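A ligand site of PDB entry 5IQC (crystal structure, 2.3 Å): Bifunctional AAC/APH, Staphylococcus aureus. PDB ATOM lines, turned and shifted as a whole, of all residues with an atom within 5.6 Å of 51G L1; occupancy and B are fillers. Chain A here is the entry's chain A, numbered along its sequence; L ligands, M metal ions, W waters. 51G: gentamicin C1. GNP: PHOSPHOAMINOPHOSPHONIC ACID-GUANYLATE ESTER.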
ATOM      1  N   TYR A  38     -28.718 -25.310  -6.049  1.00  0.00           N
ATOM      2  CA  TYR A  38     -29.708 -25.687  -7.039  1.00  0.00           C
ATOM      3  C   TYR A  38     -31.078 -25.789  -6.336  1.00  0.00           C
ATOM      4  O   TYR A  38     -32.141 -25.350  -6.810  1.00  0.00           O
ATOM      5  CB  TYR A  38     -29.265 -27.026  -7.669  1.00  0.00           C
ATOM      6  CG  TYR A  38     -27.910 -27.074  -8.396  1.00  0.00           C
ATOM      7  CD1 TYR A  38     -27.531 -26.063  -9.289  1.00  0.00           C
ATOM      8  CD2 TYR A  38     -27.069 -28.196  -8.279  1.00  0.00           C
ATOM      9  CE1 TYR A  38     -26.321 -26.128  -9.987  1.00  0.00           C
ATOM     10  CE2 TYR A  38     -25.872 -28.277  -8.976  1.00  0.00           C
ATOM     11  CZ  TYR A  38     -25.490 -27.242  -9.826  1.00  0.00           C
ATOM     12  OH  TYR A  38     -24.288 -27.339 -10.506  1.00  0.00           O
ATOM     13  N   ASN A 199     -15.242 -35.097  -2.132  1.00  0.00           N
ATOM     14  CA  ASN A 199     -15.973 -35.318  -3.379  1.00  0.00           C
ATOM     15  C   ASN A 199     -16.619 -34.094  -4.023  1.00  0.00           C
ATOM     16  O   ASN A 199     -17.409 -34.232  -4.916  1.00  0.00           O
ATOM     17  CB  ASN A 199     -17.010 -36.416  -3.189  1.00  0.00           C
ATOM     18  CG  ASN A 199     -17.443 -37.033  -4.504  1.00  0.00           C
ATOM     19  OD1 ASN A 199     -16.636 -37.211  -5.427  1.00  0.00           O
ATOM     20  ND2 ASN A 199     -18.724 -37.402  -4.585  1.00  0.00           N
ATOM     21  N   ASP A 200     -16.263 -32.912  -3.541  1.00  0.00           N
ATOM     22  CA  ASP A 200     -16.619 -31.641  -4.173  1.00  0.00           C
ATOM     23  C   ASP A 200     -15.546 -30.631  -3.818  1.00  0.00           C
ATOM     24  O   ASP A 200     -15.796 -29.485  -3.432  1.00  0.00           O
ATOM     25  CB  ASP A 200     -17.978 -31.142  -3.711  1.00  0.00           C
ATOM     26  CG  ASP A 200     -18.563 -30.088  -4.638  1.00  0.00           C
ATOM     27  OD1 ASP A 200     -18.062 -29.928  -5.784  1.00  0.00           O
ATOM     28  OD2 ASP A 200     -19.555 -29.426  -4.264  1.00  0.00           O
ATOM     29  N   SER A 202     -13.265 -28.340  -4.380  1.00  0.00           N
ATOM     30  CA  SER A 202     -12.918 -27.268  -5.282  1.00  0.00           C
ATOM     31  C   SER A 202     -12.595 -26.048  -4.455  1.00  0.00           C
ATOM     32  O   SER A 202     -12.854 -26.027  -3.234  1.00  0.00           O
ATOM     33  CB  SER A 202     -14.117 -26.979  -6.189  1.00  0.00           C
ATOM     34  OG  SER A 202     -15.310 -26.863  -5.417  1.00  0.00           O
ATOM     35  N   ASN A 204     -13.661 -23.065  -4.021  1.00  0.00           N
ATOM     36  CA  ASN A 204     -14.753 -22.352  -3.363  1.00  0.00           C
ATOM     37  C   ASN A 204     -15.197 -23.040  -2.028  1.00  0.00           C
ATOM     38  O   ASN A 204     -16.092 -22.549  -1.342  1.00  0.00           O
ATOM     39  CB  ASN A 204     -15.927 -22.206  -4.309  1.00  0.00           C
ATOM     40  CG  ASN A 204     -16.632 -23.527  -4.591  1.00  0.00           C
ATOM     41  OD1 ASN A 204     -16.001 -24.556  -4.808  1.00  0.00           O
ATOM     42  ND2 ASN A 204     -17.914 -23.510  -4.549  1.00  0.00           N
ATOM     43  N   HIS A 205     -14.576 -24.172  -1.685  1.00  0.00           N
ATOM     44  CA  HIS A 205     -14.817 -24.811  -0.396  1.00  0.00           C
ATOM     45  C   HIS A 205     -13.623 -24.773   0.537  1.00  0.00           C
ATOM     46  O   HIS A 205     -13.655 -25.344   1.629  1.00  0.00           O
ATOM     47  CB  HIS A 205     -15.299 -26.247  -0.612  1.00  0.00           C
ATOM     48  CG  HIS A 205     -16.650 -26.305  -1.229  1.00  0.00           C
ATOM     49  ND1 HIS A 205     -17.033 -27.331  -2.056  1.00  0.00           N
ATOM     50  CD2 HIS A 205     -17.705 -25.447  -1.150  1.00  0.00           C
ATOM     51  CE1 HIS A 205     -18.288 -27.123  -2.455  1.00  0.00           C
ATOM     52  NE2 HIS A 205     -18.713 -25.984  -1.921  1.00  0.00           N
ATOM     53  N   ASP A 219     -18.588 -27.981   3.172  1.00  0.00           N
ATOM     54  CA  ASP A 219     -19.458 -28.621   2.176  1.00  0.00           C
ATOM     55  C   ASP A 219     -19.014 -29.996   1.827  1.00  0.00           C
ATOM     56  O   ASP A 219     -18.541 -30.276   0.719  1.00  0.00           O
ATOM     57  CB  ASP A 219     -19.630 -27.749   0.934  1.00  0.00           C
ATOM     58  CG  ASP A 219     -20.807 -28.198   0.075  1.00  0.00           C
ATOM     59  OD1 ASP A 219     -21.451 -29.201   0.460  1.00  0.00           O
ATOM     60  OD2 ASP A 219     -21.115 -27.524  -0.954  1.00  0.00           O
ATOM     61  N   ASP A 222     -21.357 -33.869  -0.581  1.00  0.00           N
ATOM     62  CA  ASP A 222     -21.287 -34.944  -1.593  1.00  0.00           C
ATOM     63  C   ASP A 222     -20.351 -36.073  -1.206  1.00  0.00           C
ATOM     64  O   ASP A 222     -20.074 -36.966  -2.016  1.00  0.00           O
ATOM     65  CB  ASP A 222     -20.887 -34.373  -2.954  1.00  0.00           C
ATOM     66  CG  ASP A 222     -21.974 -33.469  -3.547  1.00  0.00           C
ATOM     67  OD1 ASP A 222     -23.154 -33.826  -3.509  1.00  0.00           O
ATOM     68  OD2 ASP A 222     -21.653 -32.401  -4.058  1.00  0.00           O
ATOM     69  N   TYR A 234     -11.071 -31.400  -9.172  1.00  0.00           N
ATOM     70  CA  TYR A 234     -11.122 -29.968  -9.334  1.00  0.00           C
ATOM     71  C   TYR A 234      -9.774 -29.337  -9.092  1.00  0.00           C
ATOM     72  O   TYR A 234      -9.469 -28.257  -9.651  1.00  0.00           O
ATOM     73  CB  TYR A 234     -12.241 -29.385  -8.431  1.00  0.00           C
ATOM     74  CG  TYR A 234     -13.568 -30.032  -8.749  1.00  0.00           C
ATOM     75  CD1 TYR A 234     -14.059 -30.033 -10.049  1.00  0.00           C
ATOM     76  CD2 TYR A 234     -14.292 -30.725  -7.790  1.00  0.00           C
ATOM     77  CE1 TYR A 234     -15.223 -30.665 -10.370  1.00  0.00           C
ATOM     78  CE2 TYR A 234     -15.468 -31.360  -8.100  1.00  0.00           C
ATOM     79  CZ  TYR A 234     -15.914 -31.307  -9.379  1.00  0.00           C
ATOM     80  OH  TYR A 234     -17.068 -31.934  -9.671  1.00  0.00           O
ATOM     81  N   GLU A 237      -8.294 -29.211 -12.301  1.00  0.00           N
ATOM     82  CA  GLU A 237      -9.124 -28.549 -13.304  1.00  0.00           C
ATOM     83  C   GLU A 237      -8.502 -27.269 -13.849  1.00  0.00           C
ATOM     84  O   GLU A 237      -7.986 -26.429 -13.113  1.00  0.00           O
ATOM     85  CB  GLU A 237     -10.539 -28.282 -12.778  1.00  0.00           C
ATOM     86  CG  GLU A 237     -11.462 -27.600 -13.755  1.00  0.00           C
ATOM     87  CD  GLU A 237     -12.882 -27.553 -13.251  1.00  0.00           C
ATOM     88  OE1 GLU A 237     -13.477 -28.668 -13.120  1.00  0.00           O
ATOM     89  OE2 GLU A 237     -13.384 -26.408 -13.021  1.00  0.00           O
ATOM     90  N   SER A 239      -9.798 -24.145 -15.460  1.00  0.00           N
ATOM     91  CA  SER A 239     -10.961 -23.296 -15.712  1.00  0.00           C
ATOM     92  C   SER A 239     -10.817 -21.968 -14.969  1.00  0.00           C
ATOM     93  O   SER A 239      -9.899 -21.788 -14.151  1.00  0.00           O
ATOM     94  CB  SER A 239     -12.255 -23.990 -15.247  1.00  0.00           C
ATOM     95  OG  SER A 239     -12.335 -24.113 -13.824  1.00  0.00           O
ATOM     96  N   GLU A 241     -12.704 -20.836 -12.629  1.00  0.00           N
ATOM     97  CA  GLU A 241     -13.002 -21.034 -11.202  1.00  0.00           C
ATOM     98  C   GLU A 241     -11.911 -21.741 -10.406  1.00  0.00           C
ATOM     99  O   GLU A 241     -11.882 -21.659  -9.171  1.00  0.00           O
ATOM    100  CB  GLU A 241     -14.229 -21.953 -11.036  1.00  0.00           C
ATOM    101  CG  GLU A 241     -15.527 -21.365 -11.469  1.00  0.00           C
ATOM    102  CD  GLU A 241     -16.697 -22.352 -11.390  1.00  0.00           C
ATOM    103  OE1 GLU A 241     -16.507 -23.564 -11.113  1.00  0.00           O
ATOM    104  OE2 GLU A 241     -17.841 -21.878 -11.614  1.00  0.00           O
ATOM    105  N   GLU A 242     -11.049 -22.507 -11.066  1.00  0.00           N
ATOM    106  CA  GLU A 242     -10.042 -23.252 -10.343  1.00  0.00           C
ATOM    107  C   GLU A 242      -8.660 -22.710 -10.654  1.00  0.00           C
ATOM    108  O   GLU A 242      -8.475 -21.916 -11.582  1.00  0.00           O
ATOM    109  CB  GLU A 242     -10.158 -24.748 -10.641  1.00  0.00           C
ATOM    110  CG  GLU A 242     -11.548 -25.323 -10.423  1.00  0.00           C
ATOM    111  CD  GLU A 242     -12.064 -25.222  -8.981  1.00  0.00           C
ATOM    112  OE1 GLU A 242     -11.271 -25.223  -8.013  1.00  0.00           O
ATOM    113  OE2 GLU A 242     -13.292 -25.132  -8.828  1.00  0.00           O
ATOM    114  N   GLU A 271     -14.849 -34.571 -16.536  1.00  0.00           N
ATOM    115  CA  GLU A 271     -15.092 -33.346 -17.302  1.00  0.00           C
ATOM    116  C   GLU A 271     -15.911 -33.639 -18.533  1.00  0.00           C
ATOM    117  O   GLU A 271     -16.839 -32.927 -18.865  1.00  0.00           O
ATOM    118  CB  GLU A 271     -13.778 -32.667 -17.690  1.00  0.00           C
ATOM    119  CG  GLU A 271     -13.934 -31.320 -18.415  1.00  0.00           C
ATOM    120  CD  GLU A 271     -14.625 -30.307 -17.540  1.00  0.00           C
ATOM    121  OE1 GLU A 271     -14.284 -30.220 -16.341  1.00  0.00           O
ATOM    122  OE2 GLU A 271     -15.552 -29.645 -18.030  1.00  0.00           O
ATOM    123  N   TYR A 274     -19.626 -33.944 -17.733  1.00  0.00           N
ATOM    124  CA  TYR A 274     -20.324 -32.826 -17.109  1.00  0.00           C
ATOM    125  C   TYR A 274     -21.585 -32.391 -17.828  1.00  0.00           C
ATOM    126  O   TYR A 274     -22.614 -32.211 -17.207  1.00  0.00           O
ATOM    127  CB  TYR A 274     -19.340 -31.650 -16.906  1.00  0.00           C
ATOM    128  CG  TYR A 274     -19.989 -30.383 -16.386  1.00  0.00           C
ATOM    129  CD1 TYR A 274     -20.510 -30.305 -15.109  1.00  0.00           C
ATOM    130  CD2 TYR A 274     -20.096 -29.248 -17.202  1.00  0.00           C
ATOM    131  CE1 TYR A 274     -21.119 -29.130 -14.666  1.00  0.00           C
ATOM    132  CE2 TYR A 274     -20.691 -28.083 -16.783  1.00  0.00           C
ATOM    133  CZ  TYR A 274     -21.209 -28.044 -15.531  1.00  0.00           C
ATOM    134  OH  TYR A 274     -21.808 -26.901 -15.164  1.00  0.00           O
ATOM    135  N   GLU A 277     -24.120 -35.091 -17.161  1.00  0.00           N
ATOM    136  CA  GLU A 277     -24.561 -34.958 -15.768  1.00  0.00           C
ATOM    137  C   GLU A 277     -25.597 -33.853 -15.635  1.00  0.00           C
ATOM    138  O   GLU A 277     -26.599 -34.005 -14.931  1.00  0.00           O
ATOM    139  CB  GLU A 277     -23.368 -34.658 -14.857  1.00  0.00           C
ATOM    140  CG  GLU A 277     -23.710 -34.400 -13.384  1.00  0.00           C
ATOM    141  CD  GLU A 277     -22.523 -33.822 -12.575  1.00  0.00           C
ATOM    142  OE1 GLU A 277     -22.710 -33.021 -11.625  1.00  0.00           O
ATOM    143  OE2 GLU A 277     -21.365 -34.096 -12.931  1.00  0.00           O
HETATM  144  O6  51G L   1     -21.057 -27.946  -7.020  1.00  0.00           O
HETATM  145  C14 51G L   1     -21.453 -29.036  -7.862  1.00  0.00           C
HETATM  146  C15 51G L   1     -21.212 -30.384  -7.150  1.00  0.00           C
HETATM  147  N   51G L   1     -21.671 -30.239  -5.763  1.00  0.00           N
HETATM  148  C19 51G L   1     -23.074 -29.832  -5.630  1.00  0.00           C
HETATM  149  C16 51G L   1     -21.787 -31.503  -8.070  1.00  0.00           C
HETATM  150  C18 51G L   1     -21.717 -32.911  -7.461  1.00  0.00           C
HETATM  151  O5  51G L   1     -23.180 -31.181  -8.334  1.00  0.00           O
HETATM  152  C17 51G L   1     -20.959 -31.474  -9.351  1.00  0.00           C
HETATM  153  O4  51G L   1     -20.991 -30.182  -9.968  1.00  0.00           O
HETATM  154  C13 51G L   1     -20.693 -29.031  -9.196  1.00  0.00           C
HETATM  155  O3  51G L   1     -19.322 -29.064  -8.969  1.00  0.00           O
HETATM  156  C11 51G L   1     -18.602 -27.894  -9.336  1.00  0.00           C
HETATM  157  C10 51G L   1     -17.357 -27.756  -8.451  1.00  0.00           C
HETATM  158  N1  51G L   1     -17.663 -27.538  -7.018  1.00  0.00           N
HETATM  159  C9  51G L   1     -16.494 -26.617  -8.975  1.00  0.00           C
HETATM  160  C8  51G L   1     -16.117 -26.901 -10.436  1.00  0.00           C
HETATM  161  N2  51G L   1     -15.228 -25.856 -10.934  1.00  0.00           N
HETATM  162  C12 51G L   1     -18.263 -28.162 -10.790  1.00  0.00           C
HETATM  163  O2  51G L   1     -19.433 -28.230 -11.577  1.00  0.00           O
HETATM  164  C7  51G L   1     -17.382 -27.023 -11.296  1.00  0.00           C
HETATM  165  O1  51G L   1     -16.886 -27.420 -12.584  1.00  0.00           O
HETATM  166  C6  51G L   1     -17.730 -27.544 -13.701  1.00  0.00           C
HETATM  167  C5  51G L   1     -16.868 -27.938 -14.901  1.00  0.00           C
HETATM  168  N3  51G L   1     -16.022 -29.101 -14.575  1.00  0.00           N
HETATM  169  C4  51G L   1     -16.049 -26.779 -15.467  1.00  0.00           C
HETATM  170  C3  51G L   1     -16.861 -25.480 -15.591  1.00  0.00           C
HETATM  171  O   51G L   1     -18.407 -26.320 -13.934  1.00  0.00           O
HETATM  172  C2  51G L   1     -17.581 -25.204 -14.273  1.00  0.00           C
HETATM  173  C1  51G L   1     -18.567 -23.961 -14.203  1.00  0.00           C
HETATM  174  C   51G L   1     -19.661 -23.962 -15.259  1.00  0.00           C
HETATM  175  N4  51G L   1     -19.134 -24.022 -12.843  1.00  0.00           N
HETATM  176  C20 51G L   1     -20.205 -23.053 -12.586  1.00  0.00           C
HETATM  177  PG  GNP L   2     -23.127 -26.187  -3.100  1.00  0.00           P
HETATM  178  O1G GNP L   2     -23.484 -25.977  -4.498  1.00  0.00           O
HETATM  179  O2G GNP L   2     -21.716 -25.478  -2.838  1.00  0.00           O
HETATM  180  O3G GNP L   2     -22.945 -27.729  -2.898  1.00  0.00           O
HETATM  181  N3B GNP L   2     -24.244 -25.617  -2.036  1.00  0.00           N
HETATM  182  PB  GNP L   2     -24.519 -26.031  -0.473  1.00  0.00           P
HETATM  183  O1B GNP L   2     -25.910 -26.169  -0.127  1.00  0.00           O
HETATM  184  O2B GNP L   2     -23.844 -27.415  -0.176  1.00  0.00           O
HETATM  185  O3A GNP L   2     -23.828 -24.960   0.444  1.00  0.00           O
HETATM  186  PA  GNP L   2     -22.365 -24.786   1.067  1.00  0.00           P
HETATM  187  O1A GNP L   2     -22.181 -25.916   2.147  1.00  0.00           O
HETATM  188  O2A GNP L   2     -21.332 -24.821   0.003  1.00  0.00           O
HETATM  189  O5' GNP L   2     -22.452 -23.300   1.669  1.00  0.00           O
HETATM  190  C5' GNP L   2     -22.957 -22.293   0.797  1.00  0.00           C
HETATM  191  C4' GNP L   2     -22.114 -21.075   1.026  1.00  0.00           C
HETATM  192  O4' GNP L   2     -22.225 -20.702   2.416  1.00  0.00           O
HETATM  193  C3' GNP L   2     -20.632 -21.254   0.834  1.00  0.00           C
HETATM  194  O3' GNP L   2     -20.268 -21.079  -0.513  1.00  0.00           O
HETATM  195  C2' GNP L   2     -20.087 -20.099   1.671  1.00  0.00           C
HETATM  196  O2' GNP L   2     -20.420 -18.883   1.040  1.00  0.00           O
HETATM  197  C1' GNP L   2     -21.008 -20.160   2.871  1.00  0.00           C
HETATM  198  N9  GNP L   2     -20.508 -21.001   3.956  1.00  0.00           N
HETATM  199  C8  GNP L   2     -20.960 -22.220   4.379  1.00  0.00           C
HETATM  200  N7  GNP L   2     -20.352 -22.656   5.451  1.00  0.00           N
HETATM  201  C5  GNP L   2     -19.409 -21.674   5.721  1.00  0.00           C
HETATM  202  C6  GNP L   2     -18.433 -21.585   6.753  1.00  0.00           C
HETATM  203  O6  GNP L   2     -18.279 -22.357   7.704  1.00  0.00           O
HETATM  204  N1  GNP L   2     -17.670 -20.434   6.631  1.00  0.00           N
HETATM  205  C2  GNP L   2     -17.855 -19.452   5.688  1.00  0.00           C
HETATM  206  N2  GNP L   2     -17.097 -18.358   5.784  1.00  0.00           N
HETATM  207  N3  GNP L   2     -18.789 -19.509   4.734  1.00  0.00           N
HETATM  208  C4  GNP L   2     -19.505 -20.646   4.799  1.00  0.00           C
HETATM  209 MG    MG M   1     -22.674 -28.785  -1.345  1.00  0.00          MG
HETATM  210  O   HOH W   1     -19.792 -26.401  -5.140  1.00  0.00           O
HETATM  211  O   HOH W   2     -19.208 -25.272  -7.282  1.00  0.00           O
HETATM  212  O   HOH W   3     -21.223 -30.175  -2.386  1.00  0.00           O
HETATM  213  O   HOH W   4     -23.066 -25.970  -7.317  1.00  0.00           O
HETATM  214  O   HOH W   5     -17.316 -31.499 -13.349  1.00  0.00           O
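A nitrogen (N2) of 51G L1 is in salt-bridge range of the side-chain carboxylate (OE2) of Glu 237, at 2.8 Å.
OE2 of Glu 242 lies within salt-bridge range of N2 of 51G L1 (3.0 Å).
N1 of 51G L1 sits at hydrogen-bond distance from OG of Ser 202 (2.9 Å).
N of 51G L1 is in salt-bridge range of OD2 of Asp 222 (2.8 Å).
The side-chain carboxylate (OE1) of Glu 271 lies within salt-bridge range of a nitrogen (N3) of 51G L1 (2.7 Å).
A nitrogen (N2) of 51G L1 is in salt-bridge range of the side-chain carboxylate (OE1) of Glu 241.
The side-chain carboxylate of Asp 200 lies within salt-bridge range of a nitrogen (N) of 51G L1.
The side-chain hydroxyl (OG) of Ser 202 sits at hydrogen-bond distance from the side-chain amide oxygen (OD1) of Asn 204 (2.5 Å).
O of Asp 222 sits at hydrogen-bond distance from ND2 of Asn 199 (2.9 Å).
A ring nitrogen (ND1) of His 205 sits at hydrogen-bond distance from the backbone carbonyl oxygen (O) of Asp 200 (2.8 Å).
OG of Ser 202 sits at hydrogen-bond distance from O of Asp 200 (3.3 Å).
OE2 of Glu 237 lies within hydrogen-bond range of OG of Ser 239, 2.6 Å away.
N of Glu 242 sits at hydrogen-bond distance from OG of Ser 239, at 3.4 Å.
OH of Tyr 234 touches O3 of 51G L1 (3.7 Å).
CE1 of Tyr 274 touches O2 of 51G L1, at 3.6 Å.
Glu 277 touches 51G L1 (OE1 to C17, 3.3 Å).
Within 4 Å of 51G L1: Asp 200, Ser 202, Asp 222, Tyr 234, Glu 237, Glu 241, Glu 242, Glu 271, Tyr 274 and Glu 277.
Water W1 lies within hydrogen-bond range of an oxygen (O6) of 51G L1, the side-chain carboxylate (OD2) of Asp 200 and the side-chain amide nitrogen (ND2) of Asn 204.
Water W2 bridges a nitrogen (N1) of 51G L1 (2.8 Å) and the side-chain amide nitrogen (ND2) of Asn 204 (3.5 Å).
Water W4 bridges an oxygen (O6) of 51G L1 (2.8 Å) and an oxygen (O1G) of GNP L2 (2.8 Å).
Water W3 lies within hydrogen-bond range of OD2 of Asp 200 (2.6 Å), OD2 of Asp 222 (2.8 Å) and N of 51G L1 (3.4 Å).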
